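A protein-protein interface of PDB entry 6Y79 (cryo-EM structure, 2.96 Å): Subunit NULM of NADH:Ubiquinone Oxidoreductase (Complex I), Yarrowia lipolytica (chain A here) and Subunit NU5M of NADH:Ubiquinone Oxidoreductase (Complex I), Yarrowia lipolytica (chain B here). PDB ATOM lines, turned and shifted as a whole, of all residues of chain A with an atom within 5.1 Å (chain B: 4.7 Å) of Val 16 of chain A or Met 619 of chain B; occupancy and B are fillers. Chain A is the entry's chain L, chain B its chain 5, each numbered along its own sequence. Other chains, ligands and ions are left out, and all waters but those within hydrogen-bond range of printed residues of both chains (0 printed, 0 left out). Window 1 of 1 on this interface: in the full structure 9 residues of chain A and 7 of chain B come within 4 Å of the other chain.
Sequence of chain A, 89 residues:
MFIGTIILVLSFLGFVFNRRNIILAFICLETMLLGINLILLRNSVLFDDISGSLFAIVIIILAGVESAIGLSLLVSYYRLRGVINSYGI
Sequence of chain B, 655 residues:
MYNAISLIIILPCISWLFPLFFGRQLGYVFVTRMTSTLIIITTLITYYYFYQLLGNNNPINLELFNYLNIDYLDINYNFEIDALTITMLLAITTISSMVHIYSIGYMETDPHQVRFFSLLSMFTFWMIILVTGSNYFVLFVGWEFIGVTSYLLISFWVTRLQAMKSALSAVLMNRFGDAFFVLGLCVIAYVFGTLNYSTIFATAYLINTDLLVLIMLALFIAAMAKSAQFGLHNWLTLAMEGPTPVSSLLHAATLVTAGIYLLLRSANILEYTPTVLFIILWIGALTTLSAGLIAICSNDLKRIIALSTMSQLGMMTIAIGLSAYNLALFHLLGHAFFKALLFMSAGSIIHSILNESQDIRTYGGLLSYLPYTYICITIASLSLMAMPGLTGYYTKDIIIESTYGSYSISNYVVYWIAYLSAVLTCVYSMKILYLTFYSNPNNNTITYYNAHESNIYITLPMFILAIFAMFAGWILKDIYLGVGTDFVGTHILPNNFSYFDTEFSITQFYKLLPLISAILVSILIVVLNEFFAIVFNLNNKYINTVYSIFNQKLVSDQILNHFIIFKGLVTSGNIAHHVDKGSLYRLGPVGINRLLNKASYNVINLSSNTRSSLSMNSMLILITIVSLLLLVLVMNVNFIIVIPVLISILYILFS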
ATOM      1  N   PHE A  12      23.806 -27.656  24.243  1.00  0.00           N
ATOM      2  CA  PHE A  12      23.278 -26.321  24.483  1.00  0.00           C
ATOM      3  C   PHE A  12      22.882 -26.128  25.936  1.00  0.00           C
ATOM      4  O   PHE A  12      23.227 -25.118  26.552  1.00  0.00           O
ATOM      5  CB  PHE A  12      22.080 -26.094  23.567  1.00  0.00           C
ATOM      6  CG  PHE A  12      21.479 -24.747  23.681  1.00  0.00           C
ATOM      7  CD1 PHE A  12      22.230 -23.616  23.414  1.00  0.00           C
ATOM      8  CD2 PHE A  12      20.157 -24.603  24.038  1.00  0.00           C
ATOM      9  CE1 PHE A  12      21.669 -22.365  23.516  1.00  0.00           C
ATOM     10  CE2 PHE A  12      19.591 -23.357  24.138  1.00  0.00           C
ATOM     11  CZ  PHE A  12      20.347 -22.237  23.878  1.00  0.00           C
ATOM     12  N   LEU A  13      22.175 -27.101  26.509  1.00  0.00           N
ATOM     13  CA  LEU A  13      21.741 -26.973  27.894  1.00  0.00           C
ATOM     14  C   LEU A  13      22.896 -27.124  28.870  1.00  0.00           C
ATOM     15  O   LEU A  13      22.860 -26.541  29.954  1.00  0.00           O
ATOM     16  CB  LEU A  13      20.647 -27.987  28.196  1.00  0.00           C
ATOM     17  CG  LEU A  13      19.412 -27.752  27.338  1.00  0.00           C
ATOM     18  CD1 LEU A  13      18.375 -28.818  27.583  1.00  0.00           C
ATOM     19  CD2 LEU A  13      18.861 -26.378  27.612  1.00  0.00           C
ATOM     20  N   GLY A  14      23.924 -27.892  28.515  1.00  0.00           N
ATOM     21  CA  GLY A  14      25.121 -27.911  29.331  1.00  0.00           C
ATOM     22  C   GLY A  14      25.891 -26.611  29.259  1.00  0.00           C
ATOM     23  O   GLY A  14      26.551 -26.226  30.226  1.00  0.00           O
ATOM     24  N   PHE A  15      25.828 -25.928  28.115  1.00  0.00           N
ATOM     25  CA  PHE A  15      26.396 -24.589  28.018  1.00  0.00           C
ATOM     26  C   PHE A  15      25.625 -23.601  28.879  1.00  0.00           C
ATOM     27  O   PHE A  15      26.226 -22.746  29.540  1.00  0.00           O
ATOM     28  CB  PHE A  15      26.391 -24.127  26.561  1.00  0.00           C
ATOM     29  CG  PHE A  15      27.020 -22.778  26.340  1.00  0.00           C
ATOM     30  CD1 PHE A  15      28.371 -22.669  26.104  1.00  0.00           C
ATOM     31  CD2 PHE A  15      26.260 -21.620  26.352  1.00  0.00           C
ATOM     32  CE1 PHE A  15      28.945 -21.439  25.894  1.00  0.00           C
ATOM     33  CE2 PHE A  15      26.846 -20.403  26.180  1.00  0.00           C
ATOM     34  CZ  PHE A  15      28.181 -20.310  25.939  1.00  0.00           C
ATOM     35  N   VAL A  16      24.293 -23.677  28.839  1.00  0.00           N
ATOM     36  CA  VAL A  16      23.442 -22.657  29.446  1.00  0.00           C
ATOM     37  C   VAL A  16      23.546 -22.707  30.966  1.00  0.00           C
ATOM     38  O   VAL A  16      23.734 -21.681  31.629  1.00  0.00           O
ATOM     39  CB  VAL A  16      21.990 -22.840  28.966  1.00  0.00           C
ATOM     40  CG1 VAL A  16      21.027 -22.144  29.871  1.00  0.00           C
ATOM     41  CG2 VAL A  16      21.826 -22.317  27.565  1.00  0.00           C
ATOM     42  N   PHE A  17      23.467 -23.904  31.534  1.00  0.00           N
ATOM     43  CA  PHE A  17      23.506 -24.093  32.973  1.00  0.00           C
ATOM     44  C   PHE A  17      24.908 -24.358  33.492  1.00  0.00           C
ATOM     45  O   PHE A  17      25.065 -24.899  34.590  1.00  0.00           O
ATOM     46  CB  PHE A  17      22.543 -25.209  33.362  1.00  0.00           C
ATOM     47  CG  PHE A  17      21.126 -24.894  33.010  1.00  0.00           C
ATOM     48  CD1 PHE A  17      20.378 -24.068  33.819  1.00  0.00           C
ATOM     49  CD2 PHE A  17      20.564 -25.364  31.838  1.00  0.00           C
ATOM     50  CE1 PHE A  17      19.085 -23.746  33.492  1.00  0.00           C
ATOM     51  CE2 PHE A  17      19.273 -25.038  31.502  1.00  0.00           C
ATOM     52  CZ  PHE A  17      18.533 -24.229  32.335  1.00  0.00           C
ATOM     53  N   ASN A  18      25.927 -23.986  32.724  1.00  0.00           N
ATOM     54  CA  ASN A  18      27.297 -23.991  33.210  1.00  0.00           C
ATOM     55  C   ASN A  18      27.471 -22.867  34.216  1.00  0.00           C
ATOM     56  O   ASN A  18      27.329 -21.690  33.876  1.00  0.00           O
ATOM     57  CB  ASN A  18      28.268 -23.824  32.045  1.00  0.00           C
ATOM     58  CG  ASN A  18      29.724 -23.938  32.459  1.00  0.00           C
ATOM     59  OD1 ASN A  18      30.046 -24.384  33.556  1.00  0.00           O
ATOM     60  ND2 ASN A  18      30.615 -23.522  31.574  1.00  0.00           N
ATOM     61  N   ARG A  19      27.757 -23.233  35.457  1.00  0.00           N
ATOM     62  CA  ARG A  19      28.163 -22.277  36.470  1.00  0.00           C
ATOM     63  C   ARG A  19      29.495 -22.639  37.095  1.00  0.00           C
ATOM     64  O   ARG A  19      29.943 -21.940  38.008  1.00  0.00           O
ATOM     65  CB  ARG A  19      27.107 -22.173  37.574  1.00  0.00           C
ATOM     66  CG  ARG A  19      25.753 -21.746  37.078  1.00  0.00           C
ATOM     67  CD  ARG A  19      24.726 -21.871  38.162  1.00  0.00           C
ATOM     68  NE  ARG A  19      23.569 -21.035  37.891  1.00  0.00           N
ATOM     69  CZ  ARG A  19      22.372 -21.245  38.419  1.00  0.00           C
ATOM     70  NH1 ARG A  19      22.194 -22.263  39.242  1.00  0.00           N
ATOM     71  NH2 ARG A  19      21.359 -20.442  38.128  1.00  0.00           N
ATOM     72  N   SER B 615      26.559 -16.536  32.605  1.00  0.00           N
ATOM     73  CA  SER B 615      25.480 -17.459  32.940  1.00  0.00           C
ATOM     74  C   SER B 615      24.132 -16.768  32.855  1.00  0.00           C
ATOM     75  O   SER B 615      23.159 -17.354  32.368  1.00  0.00           O
ATOM     76  CB  SER B 615      25.691 -18.027  34.338  1.00  0.00           C
ATOM     77  OG  SER B 615      25.118 -17.179  35.323  1.00  0.00           O
ATOM     78  N   MET B 616      24.084 -15.510  33.307  1.00  0.00           N
ATOM     79  CA  MET B 616      22.908 -14.657  33.193  1.00  0.00           C
ATOM     80  C   MET B 616      22.442 -14.532  31.752  1.00  0.00           C
ATOM     81  O   MET B 616      21.289 -14.855  31.431  1.00  0.00           O
ATOM     82  CB  MET B 616      23.246 -13.290  33.775  1.00  0.00           C
ATOM     83  CG  MET B 616      22.252 -12.195  33.512  1.00  0.00           C
ATOM     84  SD  MET B 616      23.046 -10.608  33.826  1.00  0.00           S
ATOM     85  CE  MET B 616      23.268 -10.694  35.600  1.00  0.00           C
ATOM     86  N   ASN B 617      23.342 -14.117  30.855  1.00  0.00           N
ATOM     87  CA  ASN B 617      22.918 -13.893  29.478  1.00  0.00           C
ATOM     88  C   ASN B 617      22.680 -15.191  28.713  1.00  0.00           C
ATOM     89  O   ASN B 617      21.781 -15.246  27.869  1.00  0.00           O
ATOM     90  CB  ASN B 617      23.938 -13.019  28.769  1.00  0.00           C
ATOM     91  CG  ASN B 617      23.995 -11.635  29.349  1.00  0.00           C
ATOM     92  OD1 ASN B 617      22.976 -10.962  29.467  1.00  0.00           O
ATOM     93  ND2 ASN B 617      25.180 -11.208  29.742  1.00  0.00           N
ATOM     94  N   SER B 618      23.433 -16.257  28.997  1.00  0.00           N
ATOM     95  CA  SER B 618      23.197 -17.508  28.285  1.00  0.00           C
ATOM     96  C   SER B 618      21.972 -18.256  28.792  1.00  0.00           C
ATOM     97  O   SER B 618      21.401 -19.046  28.038  1.00  0.00           O
ATOM     98  CB  SER B 618      24.436 -18.402  28.354  1.00  0.00           C
ATOM     99  OG  SER B 618      24.769 -18.750  29.681  1.00  0.00           O
ATOM    100  N   MET B 619      21.538 -18.024  30.031  1.00  0.00           N
ATOM    101  CA  MET B 619      20.229 -18.515  30.432  1.00  0.00           C
ATOM    102  C   MET B 619      19.117 -17.664  29.851  1.00  0.00           C
ATOM    103  O   MET B 619      18.039 -18.185  29.523  1.00  0.00           O
ATOM    104  CB  MET B 619      20.115 -18.553  31.957  1.00  0.00           C
ATOM    105  CG  MET B 619      20.845 -19.711  32.621  1.00  0.00           C
ATOM    106  SD  MET B 619      20.548 -19.880  34.386  1.00  0.00           S
ATOM    107  CE  MET B 619      21.478 -18.502  35.040  1.00  0.00           C
ATOM    108  N   LEU B 620      19.388 -16.368  29.688  1.00  0.00           N
ATOM    109  CA  LEU B 620      18.441 -15.461  29.059  1.00  0.00           C
ATOM    110  C   LEU B 620      18.193 -15.806  27.596  1.00  0.00           C
ATOM    111  O   LEU B 620      17.082 -15.615  27.107  1.00  0.00           O
ATOM    112  CB  LEU B 620      18.965 -14.036  29.193  1.00  0.00           C
ATOM    113  CG  LEU B 620      18.058 -12.869  28.850  1.00  0.00           C
ATOM    114  CD1 LEU B 620      16.782 -13.013  29.617  1.00  0.00           C
ATOM    115  CD2 LEU B 620      18.753 -11.586  29.223  1.00  0.00           C
ATOM    116  N   ILE B 621      19.206 -16.305  26.882  1.00  0.00           N
ATOM    117  CA  ILE B 621      18.988 -16.752  25.504  1.00  0.00           C
ATOM    118  C   ILE B 621      18.106 -17.996  25.469  1.00  0.00           C
ATOM    119  O   ILE B 621      17.246 -18.130  24.589  1.00  0.00           O
ATOM    120  CB  ILE B 621      20.334 -16.997  24.789  1.00  0.00           C
ATOM    121  CG1 ILE B 621      21.139 -15.705  24.715  1.00  0.00           C
ATOM    122  CG2 ILE B 621      20.133 -17.549  23.375  1.00  0.00           C
ATOM    123  CD1 ILE B 621      22.361 -15.790  23.843  1.00  0.00           C
ATOM    124  N   LEU B 622      18.280 -18.900  26.437  1.00  0.00           N
ATOM    125  CA  LEU B 622      17.472 -20.114  26.500  1.00  0.00           C
ATOM    126  C   LEU B 622      16.008 -19.792  26.752  1.00  0.00           C
ATOM    127  O   LEU B 622      15.122 -20.385  26.116  1.00  0.00           O
ATOM    128  CB  LEU B 622      17.995 -21.039  27.599  1.00  0.00           C
ATOM    129  CG  LEU B 622      17.080 -22.223  27.913  1.00  0.00           C
ATOM    130  CD1 LEU B 622      17.048 -23.173  26.744  1.00  0.00           C
ATOM    131  CD2 LEU B 622      17.473 -22.930  29.168  1.00  0.00           C
ATOM    132  N   ILE B 623      15.749 -18.845  27.668  1.00  0.00           N
ATOM    133  CA  ILE B 623      14.379 -18.511  28.065  1.00  0.00           C
ATOM    134  C   ILE B 623      13.559 -18.046  26.871  1.00  0.00           C
ATOM    135  O   ILE B 623      12.425 -18.485  26.683  1.00  0.00           O
ATOM    136  CB  ILE B 623      14.373 -17.455  29.185  1.00  0.00           C
ATOM    137  CG1 ILE B 623      14.906 -18.034  30.482  1.00  0.00           C
ATOM    138  CG2 ILE B 623      12.965 -16.927  29.432  1.00  0.00           C
ATOM    139  CD1 ILE B 623      14.920 -17.028  31.580  1.00  0.00           C
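The backbone carbonyl oxygen (O) of Ser 615 of chain B sits at hydrogen-bond distance from the side-chain hydroxyl (OG) of Ser 618 of chain B, at 3.4 Å.
Phe 12 of chain A touches Leu 622 of chain B (CE2 to CD1, 3.6 Å). Leu 13 of chain A touches Leu 622 of chain B. Phe 15 of chain A touches Ser 618 of chain B (CE2 to CB, 3.8 Å). Val 16 of chain A touches Ser 618 of chain B. Met 619 of chain B touches Val 16 of chain A. CG1 of Val 16 of chain A touches CD2 of Leu 622 of chain B, at 3.7 Å. Leu 622 of chain B touches Phe 17 of chain A (CD2 to CZ, 3.6 Å). Arg 19 of chain A touches Met 619 of chain B (NH2 to CE, 3.6 Å).
Val 16 of chain A touches just these residues of chain B: Ser 618, Met 619 and Leu 622. Of the printed residues of chain A, Ser 618 of chain B touches Phe 15 and Val 16. Printed residues of chain A within 4 Å of Leu 622 of chain B: Phe 12 (3.6 Å), Leu 13 (3.8 Å), Val 16 (3.7 Å) and Phe 17 (3.6 Å). Of the printed residues of chain B, Leu 13 of chain A touches Leu 622. Of the printed residues of chain B, Phe 17 of chain A touches Leu 622 (3.6 Å). The nearest residue of chain B that does not touch Val 16 of chain A is Ser 615 of chain B (4.4 Å). The nearest residue of chain A that does not touch Met 619 of chain B is Phe 17 of chain A (4.2 Å). The nearest printed residue of chain B that does not touch Phe 12 of chain A is Ile 621 of chain B (4.7 Å).
Along chain A the printed residues that touch a printed residue of chain B span positions 12 to 19. Among the printed residues, 8 pairs touch across the chains.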
